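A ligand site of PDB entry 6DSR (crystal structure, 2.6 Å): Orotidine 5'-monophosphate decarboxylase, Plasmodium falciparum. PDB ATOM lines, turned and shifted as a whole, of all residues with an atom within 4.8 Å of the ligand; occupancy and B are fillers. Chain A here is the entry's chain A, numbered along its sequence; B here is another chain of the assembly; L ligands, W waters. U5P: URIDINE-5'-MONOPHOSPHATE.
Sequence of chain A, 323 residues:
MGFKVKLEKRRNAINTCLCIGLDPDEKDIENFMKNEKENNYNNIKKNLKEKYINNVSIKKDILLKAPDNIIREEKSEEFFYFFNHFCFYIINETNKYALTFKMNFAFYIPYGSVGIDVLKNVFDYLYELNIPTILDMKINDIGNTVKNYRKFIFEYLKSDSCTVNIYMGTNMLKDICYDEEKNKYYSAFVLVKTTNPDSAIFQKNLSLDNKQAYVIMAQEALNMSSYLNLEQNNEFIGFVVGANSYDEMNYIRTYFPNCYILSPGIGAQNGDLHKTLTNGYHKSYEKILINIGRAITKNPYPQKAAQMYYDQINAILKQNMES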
ATOM      1  N   ASP A  23       1.795  -3.433   9.469  1.00  0.00           N
ATOM      2  CA  ASP A  23       2.053  -4.192   8.246  1.00  0.00           C
ATOM      3  C   ASP A  23       0.719  -4.675   7.685  1.00  0.00           C
ATOM      4  O   ASP A  23       0.379  -5.864   7.830  1.00  0.00           O
ATOM      5  CB  ASP A  23       2.970  -5.382   8.500  1.00  0.00           C
ATOM      6  CG  ASP A  23       4.348  -4.977   9.013  1.00  0.00           C
ATOM      7  OD1 ASP A  23       4.749  -3.802   8.813  1.00  0.00           O
ATOM      8  OD2 ASP A  23       5.022  -5.839   9.600  1.00  0.00           O
ATOM      9  N   LYS A 102       6.850   0.988  13.576  1.00  0.00           N
ATOM     10  CA  LYS A 102       7.706   0.369  12.565  1.00  0.00           C
ATOM     11  C   LYS A 102       6.828  -0.139  11.435  1.00  0.00           C
ATOM     12  O   LYS A 102       5.825  -0.811  11.679  1.00  0.00           O
ATOM     13  CB  LYS A 102       8.528  -0.787  13.142  1.00  0.00           C
ATOM     14  CG  LYS A 102       9.512  -1.374  12.124  1.00  0.00           C
ATOM     15  CD  LYS A 102      10.410  -2.454  12.738  1.00  0.00           C
ATOM     16  CE  LYS A 102       9.637  -3.739  12.998  1.00  0.00           C
ATOM     17  NZ  LYS A 102       9.437  -4.570  11.772  1.00  0.00           N
ATOM     18  N   ASN A 104       6.886  -2.059   7.596  1.00  0.00           N
ATOM     19  CA  ASN A 104       7.710  -2.855   6.720  1.00  0.00           C
ATOM     20  C   ASN A 104       7.357  -2.508   5.272  1.00  0.00           C
ATOM     21  O   ASN A 104       6.195  -2.620   4.869  1.00  0.00           O
ATOM     22  CB  ASN A 104       7.534  -4.332   7.007  1.00  0.00           C
ATOM     23  CG  ASN A 104       8.510  -5.192   6.236  1.00  0.00           C
ATOM     24  OD1 ASN A 104       8.771  -4.943   5.065  1.00  0.00           O
ATOM     25  ND2 ASN A 104       9.064  -6.201   6.903  1.00  0.00           N
ATOM     26  N   PHE A 107       4.906  -4.512   2.626  1.00  0.00           N
ATOM     27  CA  PHE A 107       3.443  -4.495   2.595  1.00  0.00           C
ATOM     28  C   PHE A 107       2.875  -3.332   1.810  1.00  0.00           C
ATOM     29  O   PHE A 107       1.677  -3.350   1.490  1.00  0.00           O
ATOM     30  CB  PHE A 107       2.871  -4.482   4.014  1.00  0.00           C
ATOM     31  CG  PHE A 107       3.072  -5.770   4.752  1.00  0.00           C
ATOM     32  CD1 PHE A 107       4.291  -6.074   5.341  1.00  0.00           C
ATOM     33  CD2 PHE A 107       2.059  -6.713   4.795  1.00  0.00           C
ATOM     34  CE1 PHE A 107       4.477  -7.281   6.002  1.00  0.00           C
ATOM     35  CE2 PHE A 107       2.235  -7.912   5.451  1.00  0.00           C
ATOM     36  CZ  PHE A 107       3.445  -8.204   6.058  1.00  0.00           C
ATOM     37  N   ASP A 136      11.010  -0.585   8.002  1.00  0.00           N
ATOM     38  CA  ASP A 136      11.653  -1.891   7.886  1.00  0.00           C
ATOM     39  C   ASP A 136      11.747  -2.207   6.398  1.00  0.00           C
ATOM     40  O   ASP A 136      10.839  -2.791   5.806  1.00  0.00           O
ATOM     41  CB  ASP A 136      10.879  -2.939   8.660  1.00  0.00           C
ATOM     42  CG  ASP A 136      11.711  -4.167   8.946  1.00  0.00           C
ATOM     43  OD1 ASP A 136      12.812  -4.294   8.380  1.00  0.00           O
ATOM     44  OD2 ASP A 136      11.235  -5.021   9.726  1.00  0.00           O
ATOM     45  N   LYS A 138      15.180  -3.142   5.135  1.00  0.00           N
ATOM     46  CA  LYS A 138      16.347  -4.010   5.016  1.00  0.00           C
ATOM     47  C   LYS A 138      17.130  -3.734   3.729  1.00  0.00           C
ATOM     48  O   LYS A 138      17.418  -4.631   2.946  1.00  0.00           O
ATOM     49  CB  LYS A 138      15.937  -5.479   5.099  1.00  0.00           C
ATOM     50  CG  LYS A 138      14.782  -5.719   6.039  1.00  0.00           C
ATOM     51  CD  LYS A 138      14.368  -7.173   6.116  1.00  0.00           C
ATOM     52  CE  LYS A 138      13.804  -7.507   7.501  1.00  0.00           C
ATOM     53  NZ  LYS A 138      12.327  -7.280   7.613  1.00  0.00           N
ATOM     54  N   LEU A 191      20.771  -5.783  10.491  1.00  0.00           N
ATOM     55  CA  LEU A 191      20.323  -7.131  10.776  1.00  0.00           C
ATOM     56  C   LEU A 191      21.472  -7.915  11.405  1.00  0.00           C
ATOM     57  O   LEU A 191      22.533  -8.073  10.783  1.00  0.00           O
ATOM     58  CB  LEU A 191      19.841  -7.807   9.491  1.00  0.00           C
ATOM     59  CG  LEU A 191      18.723  -7.076   8.757  1.00  0.00           C
ATOM     60  CD1 LEU A 191      18.387  -7.772   7.433  1.00  0.00           C
ATOM     61  CD2 LEU A 191      17.478  -6.929   9.621  1.00  0.00           C
ATOM     62  N   LYS A 193      20.758 -10.830  14.230  1.00  0.00           N
ATOM     63  CA  LYS A 193      20.219 -12.167  14.370  1.00  0.00           C
ATOM     64  C   LYS A 193      18.717 -12.064  14.128  1.00  0.00           C
ATOM     65  O   LYS A 193      18.031 -11.255  14.763  1.00  0.00           O
ATOM     66  CB  LYS A 193      20.533 -12.753  15.760  1.00  0.00           C
ATOM     67  CG  LYS A 193      20.250 -14.229  15.850  1.00  0.00           C
ATOM     68  CD  LYS A 193      21.504 -14.995  15.488  1.00  0.00           C
ATOM     69  CE  LYS A 193      21.208 -16.359  14.899  1.00  0.00           C
ATOM     70  NZ  LYS A 193      19.951 -16.900  15.415  1.00  0.00           N
ATOM     71  N   THR A 194      18.203 -12.867  13.202  1.00  0.00           N
ATOM     72  CA  THR A 194      16.844 -12.686  12.719  1.00  0.00           C
ATOM     73  C   THR A 194      15.964 -13.867  13.132  1.00  0.00           C
ATOM     74  O   THR A 194      16.448 -14.956  13.453  1.00  0.00           O
ATOM     75  CB  THR A 194      16.802 -12.525  11.186  1.00  0.00           C
ATOM     76  OG1 THR A 194      17.446 -13.641  10.549  1.00  0.00           O
ATOM     77  CG2 THR A 194      17.497 -11.241  10.771  1.00  0.00           C
ATOM     78  N   THR A 195      14.653 -13.601  13.118  1.00  0.00           N
ATOM     79  CA  THR A 195      13.640 -14.530  13.603  1.00  0.00           C
ATOM     80  C   THR A 195      13.335 -15.654  12.610  1.00  0.00           C
ATOM     81  O   THR A 195      12.381 -16.405  12.835  1.00  0.00           O
ATOM     82  CB  THR A 195      12.345 -13.776  13.926  1.00  0.00           C
ATOM     83  OG1 THR A 195      11.723 -13.334  12.715  1.00  0.00           O
ATOM     84  CG2 THR A 195      12.643 -12.576  14.793  1.00  0.00           C
ATOM     85  N   ASN A 196      14.086 -15.763  11.523  1.00  0.00           N
ATOM     86  CA  ASN A 196      13.911 -16.890  10.626  1.00  0.00           C
ATOM     87  C   ASN A 196      14.232 -18.174  11.387  1.00  0.00           C
ATOM     88  O   ASN A 196      15.121 -18.178  12.253  1.00  0.00           O
ATOM     89  CB  ASN A 196      14.834 -16.772   9.408  1.00  0.00           C
ATOM     90  CG  ASN A 196      14.666 -15.461   8.660  1.00  0.00           C
ATOM     91  OD1 ASN A 196      14.993 -14.394   9.169  1.00  0.00           O
ATOM     92  ND2 ASN A 196      14.158 -15.533   7.430  1.00  0.00           N
ATOM     93  N   VAL A 240      19.244  -5.357  14.972  1.00  0.00           N
ATOM     94  CA  VAL A 240      17.992  -6.111  14.920  1.00  0.00           C
ATOM     95  C   VAL A 240      18.289  -7.489  15.469  1.00  0.00           C
ATOM     96  O   VAL A 240      19.048  -8.259  14.877  1.00  0.00           O
ATOM     97  CB  VAL A 240      17.431  -6.191  13.488  1.00  0.00           C
ATOM     98  CG1 VAL A 240      16.183  -7.039  13.470  1.00  0.00           C
ATOM     99  CG2 VAL A 240      17.114  -4.807  12.950  1.00  0.00           C
ATOM    100  N   PRO A 264      11.986  -7.868  16.901  1.00  0.00           N
ATOM    101  CA  PRO A 264      10.666  -8.360  16.489  1.00  0.00           C
ATOM    102  C   PRO A 264      10.551  -9.858  16.755  1.00  0.00           C
ATOM    103  O   PRO A 264      11.548 -10.514  17.066  1.00  0.00           O
ATOM    104  CB  PRO A 264      10.625  -8.040  14.990  1.00  0.00           C
ATOM    105  CG  PRO A 264      12.070  -7.973  14.564  1.00  0.00           C
ATOM    106  CD  PRO A 264      12.955  -7.948  15.799  1.00  0.00           C
ATOM    107  N   ILE A 266       7.793 -11.172  18.796  1.00  0.00           N
ATOM    108  CA  ILE A 266       6.839 -11.405  19.868  1.00  0.00           C
ATOM    109  C   ILE A 266       5.439 -11.290  19.288  1.00  0.00           C
ATOM    110  O   ILE A 266       5.145 -10.384  18.499  1.00  0.00           O
ATOM    111  CB  ILE A 266       7.054 -10.395  21.025  1.00  0.00           C
ATOM    112  CG1 ILE A 266       8.306 -10.751  21.835  1.00  0.00           C
ATOM    113  CG2 ILE A 266       5.834 -10.345  21.935  1.00  0.00           C
ATOM    114  CD1 ILE A 266       8.257 -12.139  22.442  1.00  0.00           C
ATOM    115  N   ALA A 268       3.074 -12.765  16.762  1.00  0.00           N
ATOM    116  CA  ALA A 268       2.752 -13.614  15.623  1.00  0.00           C
ATOM    117  C   ALA A 268       3.740 -14.768  15.458  1.00  0.00           C
ATOM    118  O   ALA A 268       3.396 -15.796  14.864  1.00  0.00           O
ATOM    119  CB  ALA A 268       2.710 -12.774  14.341  1.00  0.00           C
ATOM    120  N   GLN A 269       4.969 -14.628  15.960  1.00  0.00           N
ATOM    121  CA  GLN A 269       5.939 -15.708  15.864  1.00  0.00           C
ATOM    122  C   GLN A 269       6.219 -16.370  17.209  1.00  0.00           C
ATOM    123  O   GLN A 269       7.166 -17.163  17.311  1.00  0.00           O
ATOM    124  CB  GLN A 269       7.229 -15.199  15.213  1.00  0.00           C
ATOM    125  CG  GLN A 269       6.956 -14.324  13.991  1.00  0.00           C
ATOM    126  CD  GLN A 269       8.209 -13.875  13.287  1.00  0.00           C
ATOM    127  OE1 GLN A 269       9.311 -14.362  13.553  1.00  0.00           O
ATOM    128  NE2 GLN A 269       8.063 -12.911  12.385  1.00  0.00           N
ATOM    129  N   ASN A 291       8.942  -5.030  19.212  1.00  0.00           N
ATOM    130  CA  ASN A 291       8.009  -4.842  18.114  1.00  0.00           C
ATOM    131  C   ASN A 291       6.904  -5.869  18.204  1.00  0.00           C
ATOM    132  O   ASN A 291       7.170  -7.078  18.309  1.00  0.00           O
ATOM    133  CB  ASN A 291       8.688  -4.929  16.752  1.00  0.00           C
ATOM    134  CG  ASN A 291       7.724  -4.623  15.616  1.00  0.00           C
ATOM    135  OD1 ASN A 291       7.336  -3.474  15.408  1.00  0.00           O
ATOM    136  ND2 ASN A 291       7.316  -5.663  14.880  1.00  0.00           N
ATOM    137  N   ILE A 292       5.668  -5.392  18.202  1.00  0.00           N
ATOM    138  CA  ILE A 292       4.492  -6.242  18.105  1.00  0.00           C
ATOM    139  C   ILE A 292       3.635  -5.717  16.967  1.00  0.00           C
ATOM    140  O   ILE A 292       3.246  -4.547  16.979  1.00  0.00           O
ATOM    141  CB  ILE A 292       3.706  -6.272  19.425  1.00  0.00           C
ATOM    142  CG1 ILE A 292       4.609  -6.834  20.522  1.00  0.00           C
ATOM    143  CG2 ILE A 292       2.473  -7.118  19.287  1.00  0.00           C
ATOM    144  CD1 ILE A 292       4.127  -6.594  21.904  1.00  0.00           C
ATOM    145  N   GLY A 293       3.381  -6.570  15.975  1.00  0.00           N
ATOM    146  CA  GLY A 293       2.600  -6.147  14.824  1.00  0.00           C
ATOM    147  C   GLY A 293       1.267  -6.858  14.685  1.00  0.00           C
ATOM    148  O   GLY A 293       0.240  -6.352  15.143  1.00  0.00           O
ATOM    149  N   ARG A 294       1.291  -8.042  14.064  1.00  0.00           N
ATOM    150  CA  ARG A 294       0.048  -8.752  13.748  1.00  0.00           C
ATOM    151  C   ARG A 294      -0.767  -9.062  14.997  1.00  0.00           C
ATOM    152  O   ARG A 294      -2.003  -9.085  14.930  1.00  0.00           O
ATOM    153  CB  ARG A 294       0.360 -10.029  12.983  1.00  0.00           C
ATOM    154  CG  ARG A 294       0.515  -9.835  11.489  1.00  0.00           C
ATOM    155  CD  ARG A 294       1.089 -11.072  10.824  1.00  0.00           C
ATOM    156  NE  ARG A 294       2.459 -11.340  11.271  1.00  0.00           N
ATOM    157  CZ  ARG A 294       3.158 -12.425  10.942  1.00  0.00           C
ATOM    158  NH1 ARG A 294       2.624 -13.358  10.165  1.00  0.00           N
ATOM    159  NH2 ARG A 294       4.392 -12.576  11.411  1.00  0.00           N
ATOM    160  N   ASP B 141      13.641 -10.964   3.676  1.00  0.00           N
ATOM    161  CA  ASP B 141      12.758 -10.817   4.820  1.00  0.00           C
ATOM    162  C   ASP B 141      12.232 -12.196   5.203  1.00  0.00           C
ATOM    163  O   ASP B 141      12.622 -13.192   4.599  1.00  0.00           O
ATOM    164  CB  ASP B 141      11.591  -9.864   4.507  1.00  0.00           C
ATOM    165  CG  ASP B 141      11.088  -9.138   5.736  1.00  0.00           C
ATOM    166  OD1 ASP B 141      11.051  -9.765   6.832  1.00  0.00           O
ATOM    167  OD2 ASP B 141      10.769  -7.934   5.633  1.00  0.00           O
ATOM    168  N   ILE B 142      11.358 -12.240   6.212  1.00  0.00           N
ATOM    169  CA  ILE B 142      10.745 -13.508   6.604  1.00  0.00           C
ATOM    170  C   ILE B 142       9.738 -13.950   5.538  1.00  0.00           C
ATOM    171  O   ILE B 142       9.270 -13.166   4.713  1.00  0.00           O
ATOM    172  CB  ILE B 142      10.073 -13.382   7.983  1.00  0.00           C
ATOM    173  CG1 ILE B 142       8.916 -12.388   7.900  1.00  0.00           C
ATOM    174  CG2 ILE B 142      11.094 -12.958   9.027  1.00  0.00           C
ATOM    175  CD1 ILE B 142       8.256 -12.130   9.234  1.00  0.00           C
ATOM    176  N   THR B 145       6.488 -12.042   4.936  1.00  0.00           N
ATOM    177  CA  THR B 145       6.665 -10.732   4.330  1.00  0.00           C
ATOM    178  C   THR B 145       7.107 -10.812   2.878  1.00  0.00           C
ATOM    179  O   THR B 145       6.592 -10.086   2.029  1.00  0.00           O
ATOM    180  CB  THR B 145       7.652  -9.929   5.181  1.00  0.00           C
ATOM    181  OG1 THR B 145       7.205  -9.895   6.536  1.00  0.00           O
ATOM    182  CG2 THR B 145       7.757  -8.519   4.665  1.00  0.00           C
ATOM    183  N   MET B 168      19.581 -13.777   5.553  1.00  0.00           N
ATOM    184  CA  MET B 168      18.598 -14.041   6.609  1.00  0.00           C
ATOM    185  C   MET B 168      18.134 -15.484   6.645  1.00  0.00           C
ATOM    186  O   MET B 168      17.483 -15.898   7.614  1.00  0.00           O
ATOM    187  CB  MET B 168      17.397 -13.122   6.440  1.00  0.00           C
ATOM    188  CG  MET B 168      17.596 -11.732   6.990  1.00  0.00           C
ATOM    189  SD  MET B 168      16.200 -10.712   6.506  1.00  0.00           S
ATOM    190  CE  MET B 168      15.038 -11.099   7.822  1.00  0.00           C
HETATM  191  N1  U5P L   1      11.041  -8.538  10.880  1.00  0.00           N
HETATM  192  C2  U5P L   1      10.933  -9.903  11.531  1.00  0.00           C
HETATM  193  N3  U5P L   1      12.205 -10.631  11.923  1.00  0.00           N
HETATM  194  C4  U5P L   1      13.504 -10.015  11.674  1.00  0.00           C
HETATM  195  C5  U5P L   1      13.595  -8.673  11.037  1.00  0.00           C
HETATM  196  C6  U5P L   1      12.335  -7.940  10.652  1.00  0.00           C
HETATM  197  O2  U5P L   1       9.834 -10.436  11.749  1.00  0.00           O
HETATM  198  O4  U5P L   1      14.496 -10.598  11.982  1.00  0.00           O
HETATM  199  C1' U5P L   1       9.847  -7.784  10.490  1.00  0.00           C
HETATM  200  C2' U5P L   1       8.850  -8.554   9.618  1.00  0.00           C
HETATM  201  O2' U5P L   1       9.209  -8.538   8.248  1.00  0.00           O
HETATM  202  C3' U5P L   1       7.549  -7.846   9.956  1.00  0.00           C
HETATM  203  C4' U5P L   1       7.715  -7.526  11.434  1.00  0.00           C
HETATM  204  O3' U5P L   1       7.453  -6.628   9.221  1.00  0.00           O
HETATM  205  O4' U5P L   1       9.141  -7.422  11.667  1.00  0.00           O
HETATM  206  C5' U5P L   1       7.141  -8.540  12.393  1.00  0.00           C
HETATM  207  O5' U5P L   1       5.771  -8.261  12.692  1.00  0.00           O
HETATM  208  P   U5P L   1       4.833  -9.363  13.340  1.00  0.00           P
HETATM  209  O1P U5P L   1       4.699  -9.024  14.829  1.00  0.00           O
HETATM  210  O2P U5P L   1       5.551 -10.661  13.202  1.00  0.00           O
HETATM  211  O3P U5P L   1       3.474  -9.231  12.700  1.00  0.00           O
HETATM  212  O   HOH W   1       3.732  -8.404   9.664  1.00  0.00           O
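The side-chain hydroxyl (OG1) of Thr 195 is in hydrogen-bond range of the side-chain amide oxygen (OE1) of Gln 269 (2.8 Å).
The side-chain amide oxygen of Asn 104 sits close to the backbone carbonyl oxygen of Asp 136 (3.1 Å).
OD2 of Asp 141 of chain B lies within salt-bridge range of NZ of Lys 138, at 2.6 Å.
The backbone carbonyl oxygen (O) of Val 240 is in hydrogen-bond range of the backbone NH (N) of Lys 193 (3.2 Å).
N of Asn 104 lies within hydrogen-bond range of OD1 of Asp 23 (3.0 Å).
OG1 of Thr 194 is in hydrogen-bond range of OD1 of Asn 196 (2.9 Å).
OD2 of Asp 136 lies within salt-bridge range of NZ of Lys 102, 2.8 Å away.
ND2 of Asn 104 sits at hydrogen-bond distance from OD2 of Asp 141 of chain B, at 2.7 Å.
Residues that only touch the ligand: Asp 136, Thr 194, Val 240, Pro 264, Ile 266, Ala 268, Asn 291 and Ile 142 of chain B.
The backbone NH of Gly 293 sits at hydrogen-bond distance from an oxygen (O1P) of the ligand, 3.0 Å away.
NE of Arg 294 is in salt-bridge range of O3P of the ligand.
ND2 of Asn 104 lies within hydrogen-bond range of O2' of the ligand (2.7 Å).
An oxygen (O2') of the ligand lies within hydrogen-bond range of the side-chain carboxylate (OD1) of Asp 141 of chain B (2.6 Å).
OD2 of Asp 23 sits at hydrogen-bond distance from O3' of the ligand (2.6 Å).
NZ of Lys 102 sits at hydrogen-bond distance from O4' of the ligand, 2.9 Å away.
NE2 of Gln 269 sits at hydrogen-bond distance from O2 of the ligand (3.1 Å).
OG1 of Thr 145 of chain B sits at hydrogen-bond distance from O2' of the ligand, at 3.0 Å.
A nitrogen (N3) of the ligand is in hydrogen-bond range of the side-chain hydroxyl (OG1) of Thr 195 (2.9 Å).
The backbone NH (N) of Thr 195 is in hydrogen-bond range of an oxygen (O4) of the ligand (3.2 Å).
An oxygen (O2') of the ligand lies close to the side-chain amino group (NZ) of Lys 138, 3.4 Å away.
The backbone NH (N) of Arg 294 is in hydrogen-bond range of an oxygen (O3P) of the ligand, 2.8 Å away.
Water W1 bridges the side-chain carboxylate of Asp 23 (2.9 Å) and an oxygen (O3P) of the ligand (3.2 Å).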
